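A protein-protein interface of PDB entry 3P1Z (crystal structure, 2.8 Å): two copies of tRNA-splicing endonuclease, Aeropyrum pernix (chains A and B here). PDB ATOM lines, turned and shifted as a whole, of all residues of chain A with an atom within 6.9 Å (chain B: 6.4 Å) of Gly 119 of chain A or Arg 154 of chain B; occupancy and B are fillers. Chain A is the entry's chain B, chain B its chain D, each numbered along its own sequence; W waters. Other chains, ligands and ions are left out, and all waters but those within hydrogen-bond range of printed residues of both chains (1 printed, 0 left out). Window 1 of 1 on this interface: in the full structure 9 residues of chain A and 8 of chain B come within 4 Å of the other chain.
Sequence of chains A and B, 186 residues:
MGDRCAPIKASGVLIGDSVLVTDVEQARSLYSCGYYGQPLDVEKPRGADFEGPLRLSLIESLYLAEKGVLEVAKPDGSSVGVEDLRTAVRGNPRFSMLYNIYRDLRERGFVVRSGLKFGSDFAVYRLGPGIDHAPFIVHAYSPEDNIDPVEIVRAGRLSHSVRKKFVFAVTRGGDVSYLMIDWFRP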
ATOM      1  N   GLY A 115       4.048 -25.515   4.698  1.00  0.00           N
ATOM      2  CA  GLY A 115       4.093 -24.168   4.176  1.00  0.00           C
ATOM      3  C   GLY A 115       3.089 -23.972   3.066  1.00  0.00           C
ATOM      4  O   GLY A 115       3.041 -22.911   2.473  1.00  0.00           O
ATOM      5  N   LEU A 116       2.276 -24.992   2.806  1.00  0.00           N
ATOM      6  CA  LEU A 116       1.320 -25.003   1.695  1.00  0.00           C
ATOM      7  C   LEU A 116       0.536 -23.700   1.527  1.00  0.00           C
ATOM      8  O   LEU A 116       0.559 -23.081   0.462  1.00  0.00           O
ATOM      9  CB  LEU A 116       0.326 -26.149   1.857  1.00  0.00           C
ATOM     10  CG  LEU A 116      -0.581 -26.435   0.661  1.00  0.00           C
ATOM     11  CD1 LEU A 116       0.049 -27.512  -0.203  1.00  0.00           C
ATOM     12  CD2 LEU A 116      -1.980 -26.863   1.090  1.00  0.00           C
ATOM     13  N   LYS A 117      -0.169 -23.296   2.581  1.00  0.00           N
ATOM     14  CA  LYS A 117      -0.985 -22.090   2.547  1.00  0.00           C
ATOM     15  C   LYS A 117      -0.150 -20.826   2.365  1.00  0.00           C
ATOM     16  O   LYS A 117      -0.690 -19.733   2.229  1.00  0.00           O
ATOM     17  CB  LYS A 117      -1.848 -22.014   3.811  1.00  0.00           C
ATOM     18  CG  LYS A 117      -3.044 -22.980   3.798  1.00  0.00           C
ATOM     19  CD  LYS A 117      -3.067 -23.875   5.039  1.00  0.00           C
ATOM     20  CE  LYS A 117      -1.790 -24.725   5.119  1.00  0.00           C
ATOM     21  NZ  LYS A 117      -1.594 -25.422   6.438  1.00  0.00           N
ATOM     22  N   PHE A 118       1.167 -20.977   2.354  1.00  0.00           N
ATOM     23  CA  PHE A 118       2.038 -19.847   2.074  1.00  0.00           C
ATOM     24  C   PHE A 118       2.881 -20.079   0.837  1.00  0.00           C
ATOM     25  O   PHE A 118       3.891 -19.411   0.623  1.00  0.00           O
ATOM     26  CB  PHE A 118       2.914 -19.527   3.268  1.00  0.00           C
ATOM     27  CG  PHE A 118       2.139 -19.342   4.521  1.00  0.00           C
ATOM     28  CD1 PHE A 118       1.462 -18.153   4.763  1.00  0.00           C
ATOM     29  CD2 PHE A 118       2.047 -20.372   5.449  1.00  0.00           C
ATOM     30  CE1 PHE A 118       0.718 -17.988   5.920  1.00  0.00           C
ATOM     31  CE2 PHE A 118       1.317 -20.212   6.610  1.00  0.00           C
ATOM     32  CZ  PHE A 118       0.649 -19.019   6.847  1.00  0.00           C
ATOM     33  N   GLY A 119       2.444 -21.024   0.015  1.00  0.00           N
ATOM     34  CA  GLY A 119       3.105 -21.301  -1.240  1.00  0.00           C
ATOM     35  C   GLY A 119       4.568 -21.626  -1.059  1.00  0.00           C
ATOM     36  O   GLY A 119       5.403 -21.165  -1.838  1.00  0.00           O
ATOM     37  N   SER A 120       4.871 -22.409  -0.023  1.00  0.00           N
ATOM     38  CA  SER A 120       6.226 -22.899   0.209  1.00  0.00           C
ATOM     39  C   SER A 120       6.261 -24.260   0.909  1.00  0.00           C
ATOM     40  O   SER A 120       5.249 -24.974   0.991  1.00  0.00           O
ATOM     41  CB  SER A 120       7.068 -21.883   0.981  1.00  0.00           C
ATOM     42  OG  SER A 120       6.437 -21.513   2.187  1.00  0.00           O
ATOM     43  N   ASP A 121       7.446 -24.620   1.390  1.00  0.00           N
ATOM     44  CA  ASP A 121       7.686 -25.959   1.915  1.00  0.00           C
ATOM     45  C   ASP A 121       7.250 -26.024   3.350  1.00  0.00           C
ATOM     46  O   ASP A 121       6.485 -26.899   3.712  1.00  0.00           O
ATOM     47  CB  ASP A 121       9.166 -26.336   1.804  1.00  0.00           C
ATOM     48  CG  ASP A 121       9.577 -26.710   0.387  1.00  0.00           C
ATOM     49  OD1 ASP A 121       8.687 -26.985  -0.448  1.00  0.00           O
ATOM     50  OD2 ASP A 121      10.798 -26.730   0.121  1.00  0.00           O
ATOM     51  N   ILE A 137       8.942 -18.366   6.557  1.00  0.00           N
ATOM     52  CA  ILE A 137       8.555 -19.076   5.334  1.00  0.00           C
ATOM     53  C   ILE A 137       9.795 -19.702   4.720  1.00  0.00           C
ATOM     54  O   ILE A 137      10.727 -18.998   4.377  1.00  0.00           O
ATOM     55  CB  ILE A 137       7.901 -18.130   4.308  1.00  0.00           C
ATOM     56  CG1 ILE A 137       6.742 -17.389   4.935  1.00  0.00           C
ATOM     57  CG2 ILE A 137       7.302 -18.899   3.189  1.00  0.00           C
ATOM     58  CD1 ILE A 137       5.539 -18.275   5.137  1.00  0.00           C
ATOM     59  N   HIS A 139      11.790 -22.258   1.942  1.00  0.00           N
ATOM     60  CA  HIS A 139      11.863 -23.004   0.704  1.00  0.00           C
ATOM     61  C   HIS A 139      13.130 -23.834   0.828  1.00  0.00           C
ATOM     62  O   HIS A 139      14.167 -23.319   1.253  1.00  0.00           O
ATOM     63  CB  HIS A 139      11.964 -22.046  -0.504  1.00  0.00           C
ATOM     64  CG  HIS A 139      10.996 -20.875  -0.467  1.00  0.00           C
ATOM     65  ND1 HIS A 139      11.285 -19.699   0.217  1.00  0.00           N
ATOM     66  CD2 HIS A 139       9.804 -20.701  -1.042  1.00  0.00           C
ATOM     67  CE1 HIS A 139      10.269 -18.873   0.070  1.00  0.00           C
ATOM     68  NE2 HIS A 139       9.355 -19.428  -0.691  1.00  0.00           N
ATOM     69  N   TYR A 141      16.291 -26.316  -0.524  1.00  0.00           N
ATOM     70  CA  TYR A 141      17.196 -26.493  -1.671  1.00  0.00           C
ATOM     71  C   TYR A 141      18.453 -27.280  -1.310  1.00  0.00           C
ATOM     72  O   TYR A 141      19.073 -27.032  -0.285  1.00  0.00           O
ATOM     73  CB  TYR A 141      17.690 -25.136  -2.182  1.00  0.00           C
ATOM     74  CG  TYR A 141      16.694 -24.271  -2.910  1.00  0.00           C
ATOM     75  CD1 TYR A 141      16.192 -24.646  -4.145  1.00  0.00           C
ATOM     76  CD2 TYR A 141      16.282 -23.057  -2.373  1.00  0.00           C
ATOM     77  CE1 TYR A 141      15.284 -23.849  -4.817  1.00  0.00           C
ATOM     78  CE2 TYR A 141      15.385 -22.255  -3.036  1.00  0.00           C
ATOM     79  CZ  TYR A 141      14.885 -22.653  -4.260  1.00  0.00           C
ATOM     80  OH  TYR A 141      13.990 -21.845  -4.926  1.00  0.00           O
ATOM     81  N   GLU A 151      13.743 -16.298  -9.415  1.00  0.00           N
ATOM     82  CA  GLU A 151      13.235 -17.132  -8.322  1.00  0.00           C
ATOM     83  C   GLU A 151      13.458 -16.519  -6.939  1.00  0.00           C
ATOM     84  O   GLU A 151      12.692 -16.753  -6.010  1.00  0.00           O
ATOM     85  CB  GLU A 151      13.841 -18.537  -8.400  1.00  0.00           C
ATOM     86  CG  GLU A 151      13.136 -19.425  -9.421  1.00  0.00           C
ATOM     87  CD  GLU A 151      13.786 -20.787  -9.587  1.00  0.00           C
ATOM     88  OE1 GLU A 151      13.239 -21.775  -9.045  1.00  0.00           O
ATOM     89  OE2 GLU A 151      14.845 -20.870 -10.251  1.00  0.00           O
ATOM     90  N   ARG A 154      10.493 -13.958  -7.040  1.00  0.00           N
ATOM     91  CA  ARG A 154       9.205 -14.634  -6.844  1.00  0.00           C
ATOM     92  C   ARG A 154       9.043 -14.938  -5.352  1.00  0.00           C
ATOM     93  O   ARG A 154       7.940 -14.894  -4.796  1.00  0.00           O
ATOM     94  CB  ARG A 154       9.098 -15.919  -7.695  1.00  0.00           C
ATOM     95  CG  ARG A 154       7.774 -16.695  -7.505  1.00  0.00           C
ATOM     96  CD  ARG A 154       7.723 -18.116  -8.144  1.00  0.00           C
ATOM     97  NE  ARG A 154       8.532 -19.111  -7.435  1.00  0.00           N
ATOM     98  CZ  ARG A 154       8.998 -20.233  -7.982  1.00  0.00           C
ATOM     99  NH1 ARG A 154       8.725 -20.519  -9.249  1.00  0.00           N
ATOM    100  NH2 ARG A 154       9.735 -21.074  -7.259  1.00  0.00           N
ATOM    101  N   LEU A 158       6.421 -13.800  -2.687  1.00  0.00           N
ATOM    102  CA  LEU A 158       5.620 -14.708  -1.852  1.00  0.00           C
ATOM    103  C   LEU A 158       5.554 -14.235  -0.406  1.00  0.00           C
ATOM    104  O   LEU A 158       4.533 -14.402   0.263  1.00  0.00           O
ATOM    105  CB  LEU A 158       6.112 -16.166  -1.909  1.00  0.00           C
ATOM    106  CG  LEU A 158       5.423 -17.089  -2.928  1.00  0.00           C
ATOM    107  CD1 LEU A 158       6.248 -18.352  -3.165  1.00  0.00           C
ATOM    108  CD2 LEU A 158       3.980 -17.440  -2.531  1.00  0.00           C
ATOM    109  N   TYR B 141       6.498 -23.664 -19.392  1.00  0.00           N
ATOM    110  CA  TYR B 141       6.873 -25.064 -19.100  1.00  0.00           C
ATOM    111  C   TYR B 141       7.103 -25.878 -20.373  1.00  0.00           C
ATOM    112  O   TYR B 141       6.322 -25.799 -21.323  1.00  0.00           O
ATOM    113  CB  TYR B 141       5.770 -25.780 -18.297  1.00  0.00           C
ATOM    114  CG  TYR B 141       5.794 -25.573 -16.793  1.00  0.00           C
ATOM    115  CD1 TYR B 141       6.863 -26.021 -16.026  1.00  0.00           C
ATOM    116  CD2 TYR B 141       4.736 -24.951 -16.144  1.00  0.00           C
ATOM    117  CE1 TYR B 141       6.885 -25.831 -14.668  1.00  0.00           C
ATOM    118  CE2 TYR B 141       4.753 -24.753 -14.793  1.00  0.00           C
ATOM    119  CZ  TYR B 141       5.822 -25.196 -14.055  1.00  0.00           C
ATOM    120  OH  TYR B 141       5.834 -25.009 -12.692  1.00  0.00           O
ATOM    121  N   PRO B 149       2.995 -31.756  -7.333  1.00  0.00           N
ATOM    122  CA  PRO B 149       1.617 -31.243  -7.377  1.00  0.00           C
ATOM    123  C   PRO B 149       1.361 -30.011  -6.499  1.00  0.00           C
ATOM    124  O   PRO B 149       0.449 -29.252  -6.768  1.00  0.00           O
ATOM    125  CB  PRO B 149       0.802 -32.444  -6.900  1.00  0.00           C
ATOM    126  CG  PRO B 149       1.591 -33.596  -7.388  1.00  0.00           C
ATOM    127  CD  PRO B 149       3.023 -33.220  -7.187  1.00  0.00           C
ATOM    128  N   VAL B 150       2.158 -29.819  -5.460  1.00  0.00           N
ATOM    129  CA  VAL B 150       1.930 -28.709  -4.549  1.00  0.00           C
ATOM    130  C   VAL B 150       2.219 -27.427  -5.264  1.00  0.00           C
ATOM    131  O   VAL B 150       1.739 -26.370  -4.859  1.00  0.00           O
ATOM    132  CB  VAL B 150       2.841 -28.746  -3.307  1.00  0.00           C
ATOM    133  CG1 VAL B 150       2.395 -29.808  -2.337  1.00  0.00           C
ATOM    134  CG2 VAL B 150       4.303 -28.915  -3.712  1.00  0.00           C
ATOM    135  N   GLU B 151       3.036 -27.527  -6.311  1.00  0.00           N
ATOM    136  CA  GLU B 151       3.404 -26.368  -7.107  1.00  0.00           C
ATOM    137  C   GLU B 151       2.151 -25.803  -7.769  1.00  0.00           C
ATOM    138  O   GLU B 151       1.917 -24.594  -7.733  1.00  0.00           O
ATOM    139  CB  GLU B 151       4.511 -26.724  -8.099  1.00  0.00           C
ATOM    140  CG  GLU B 151       5.914 -26.674  -7.463  1.00  0.00           C
ATOM    141  CD  GLU B 151       6.963 -27.455  -8.241  1.00  0.00           C
ATOM    142  OE1 GLU B 151       7.024 -27.285  -9.480  1.00  0.00           O
ATOM    143  OE2 GLU B 151       7.726 -28.228  -7.607  1.00  0.00           O
ATOM    144  N   ILE B 152       1.326 -26.675  -8.335  1.00  0.00           N
ATOM    145  CA  ILE B 152       0.003 -26.265  -8.787  1.00  0.00           C
ATOM    146  C   ILE B 152      -0.732 -25.389  -7.764  1.00  0.00           C
ATOM    147  O   ILE B 152      -1.332 -24.383  -8.120  1.00  0.00           O
ATOM    148  CB  ILE B 152      -0.914 -27.465  -9.060  1.00  0.00           C
ATOM    149  CG1 ILE B 152      -0.359 -28.373 -10.148  1.00  0.00           C
ATOM    150  CG2 ILE B 152      -2.316 -27.006  -9.428  1.00  0.00           C
ATOM    151  CD1 ILE B 152      -1.250 -29.565 -10.378  1.00  0.00           C
ATOM    152  N   VAL B 153      -0.727 -25.793  -6.497  1.00  0.00           N
ATOM    153  CA  VAL B 153      -1.340 -24.965  -5.464  1.00  0.00           C
ATOM    154  C   VAL B 153      -0.598 -23.629  -5.348  1.00  0.00           C
ATOM    155  O   VAL B 153      -1.223 -22.571  -5.358  1.00  0.00           O
ATOM    156  CB  VAL B 153      -1.370 -25.658  -4.076  1.00  0.00           C
ATOM    157  CG1 VAL B 153      -1.584 -24.635  -2.958  1.00  0.00           C
ATOM    158  CG2 VAL B 153      -2.422 -26.782  -4.014  1.00  0.00           C
ATOM    159  N   ARG B 154       0.731 -23.682  -5.228  1.00  0.00           N
ATOM    160  CA  ARG B 154       1.546 -22.475  -5.096  1.00  0.00           C
ATOM    161  C   ARG B 154       1.072 -21.456  -6.121  1.00  0.00           C
ATOM    162  O   ARG B 154       1.030 -20.251  -5.868  1.00  0.00           O
ATOM    163  CB  ARG B 154       3.051 -22.757  -5.284  1.00  0.00           C
ATOM    164  CG  ARG B 154       3.930 -21.465  -5.256  1.00  0.00           C
ATOM    165  CD  ARG B 154       5.451 -21.703  -5.496  1.00  0.00           C
ATOM    166  NE  ARG B 154       5.737 -22.523  -6.676  1.00  0.00           N
ATOM    167  CZ  ARG B 154       6.911 -23.105  -6.929  1.00  0.00           C
ATOM    168  NH1 ARG B 154       7.938 -22.953  -6.090  1.00  0.00           N
ATOM    169  NH2 ARG B 154       7.054 -23.838  -8.032  1.00  0.00           N
ATOM    170  N   ALA B 155       0.714 -21.967  -7.288  1.00  0.00           N
ATOM    171  CA  ALA B 155       0.175 -21.149  -8.355  1.00  0.00           C
ATOM    172  C   ALA B 155      -1.104 -20.452  -7.903  1.00  0.00           C
ATOM    173  O   ALA B 155      -1.192 -19.220  -7.906  1.00  0.00           O
ATOM    174  CB  ALA B 155      -0.097 -22.017  -9.541  1.00  0.00           C
ATOM    175  N   GLY B 156      -2.094 -21.261  -7.528  1.00  0.00           N
ATOM    176  CA  GLY B 156      -3.342 -20.785  -6.954  1.00  0.00           C
ATOM    177  C   GLY B 156      -3.091 -19.845  -5.798  1.00  0.00           C
ATOM    178  O   GLY B 156      -3.853 -18.910  -5.570  1.00  0.00           O
ATOM    179  N   ARG B 157      -2.020 -20.091  -5.053  1.00  0.00           N
ATOM    180  CA  ARG B 157      -1.526 -19.043  -4.181  1.00  0.00           C
ATOM    181  C   ARG B 157      -1.216 -17.816  -5.043  1.00  0.00           C
ATOM    182  O   ARG B 157      -2.000 -16.886  -5.069  1.00  0.00           O
ATOM    183  CB  ARG B 157      -0.305 -19.479  -3.355  1.00  0.00           C
ATOM    184  CG  ARG B 157      -0.667 -20.261  -2.093  1.00  0.00           C
ATOM    185  CD  ARG B 157      -1.905 -19.671  -1.438  1.00  0.00           C
ATOM    186  NE  ARG B 157      -2.690 -20.645  -0.681  1.00  0.00           N
ATOM    187  CZ  ARG B 157      -3.964 -20.467  -0.342  1.00  0.00           C
ATOM    188  NH1 ARG B 157      -4.595 -19.355  -0.700  1.00  0.00           N
ATOM    189  NH2 ARG B 157      -4.611 -21.397   0.344  1.00  0.00           N
ATOM    190  N   LEU B 158      -0.097 -17.819  -5.766  1.00  0.00           N
ATOM    191  CA  LEU B 158       0.330 -16.611  -6.466  1.00  0.00           C
ATOM    192  C   LEU B 158      -0.859 -15.847  -7.001  1.00  0.00           C
ATOM    193  O   LEU B 158      -0.919 -14.621  -6.910  1.00  0.00           O
ATOM    194  CB  LEU B 158       1.318 -16.921  -7.591  1.00  0.00           C
ATOM    195  CG  LEU B 158       2.755 -16.691  -7.111  1.00  0.00           C
ATOM    196  CD1 LEU B 158       3.750 -17.251  -8.097  1.00  0.00           C
ATOM    197  CD2 LEU B 158       3.021 -15.213  -6.842  1.00  0.00           C
ATOM    198  N   SER B 159      -1.818 -16.592  -7.530  1.00  0.00           N
ATOM    199  CA  SER B 159      -2.978 -16.008  -8.171  1.00  0.00           C
ATOM    200  C   SER B 159      -4.040 -15.611  -7.176  1.00  0.00           C
ATOM    201  O   SER B 159      -5.002 -14.937  -7.516  1.00  0.00           O
ATOM    202  CB  SER B 159      -3.565 -16.997  -9.155  1.00  0.00           C
ATOM    203  OG  SER B 159      -3.269 -16.586 -10.481  1.00  0.00           O
ATOM    204  N   PHE B 166      -4.654 -18.300 -13.093  1.00  0.00           N
ATOM    205  CA  PHE B 166      -3.354 -18.303 -13.744  1.00  0.00           C
ATOM    206  C   PHE B 166      -3.282 -19.408 -14.770  1.00  0.00           C
ATOM    207  O   PHE B 166      -4.007 -20.387 -14.698  1.00  0.00           O
ATOM    208  CB  PHE B 166      -2.277 -18.591 -12.720  1.00  0.00           C
ATOM    209  CG  PHE B 166      -2.418 -19.927 -12.099  1.00  0.00           C
ATOM    210  CD1 PHE B 166      -1.821 -21.044 -12.668  1.00  0.00           C
ATOM    211  CD2 PHE B 166      -3.209 -20.086 -10.966  1.00  0.00           C
ATOM    212  CE1 PHE B 166      -1.985 -22.303 -12.095  1.00  0.00           C
ATOM    213  CE2 PHE B 166      -3.381 -21.342 -10.376  1.00  0.00           C
ATOM    214  CZ  PHE B 166      -2.762 -22.453 -10.943  1.00  0.00           C
HETATM  215  O   HOH W   1      10.434 -23.667  -7.208  1.00  0.00           O
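NH1 of Arg 154 of chain B lies close to NH2 of Arg 154 of chain A, at 2.9 Å.
The guanidinium group (NH2) of Arg 154 of chain A lies within salt-bridge range of the side-chain carboxylate (OE1) of Glu 151 of chain A (3.99 Å).
The side-chain carboxylate of Glu 151 of chain B is in salt-bridge range of the guanidinium group of Arg 154 of chain B (3.7 Å).
Among the printed residues, merely in contact across the chains: Leu 116 of chain A with Val 150 of chain B (3.9 Å), Leu 116 of chain A with Arg 157 of chain B (3.998 Å), Lys 117 of chain A with Arg 157 of chain B (3.6 Å), Gly 119 of chain A with Arg 154 of chain B (3.7 Å) and Gly 119 of chain A with Arg 157 of chain B (3.8 Å).
Printed residues of chain B within 4 Å of Leu 116 of chain A: Val 150 (3.9 Å) and Arg 157 (3.998 Å).
Of the printed residues of chain B, Lys 117 of chain A touches Arg 157.
Gly 119 of chain A touches just these residues of chain B: Arg 154 and Arg 157.
Ile 137 of chain A touches none of the printed residues of chain B.
Of the printed residues of chain B, Arg 154 of chain A touches Arg 154.
Printed residues of chain A within 4 Å of Val 150 of chain B: Leu 116.
Of the printed residues of chain A, Arg 154 of chain B touches Gly 119 and Arg 154.
Printed residues of chain A within 4 Å of Arg 157 of chain B: Leu 116, Lys 117 and Gly 119.
The nearest printed residue of chain A that does not touch Val 150 of chain B is Asp 121 of chain A (5.8 Å).
Of the 13 printed residues of chain B, 3 touch a printed residue of chain A.
Printed residues of chain B that touch a printed residue of chain A: Val 150, Arg 154 and Arg 157.
Hydrophobic or aromatic side chains of chain B within 4 Å of the printed part of chain A: Val 150.
Along chain B the printed residues that touch a printed residue of chain A span positions 150 to 157.
Hydrophobic or aromatic side chains of chain A within 4 Å of the printed part of chain B: Leu 116.
Among the printed residues, 6 pairs touch across the chains.
Among the printed residues, no Asp or Glu carboxylate lies within 4 Å of a Lys or Arg side-chain nitrogen of the other chain.
Arg 154 of chain B touches its own counterpart, Arg 154 of chain A.
4 positions are printed for both chains.
Of the 6 pairs that touch across the chains among the printed residues, 1 has its exchanged pair printed and touching as well.
Water W1 bridges NH2 of Arg 154 of chain A (2.7 Å) and NH1 of Arg 154 of chain B (2.8 Å).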
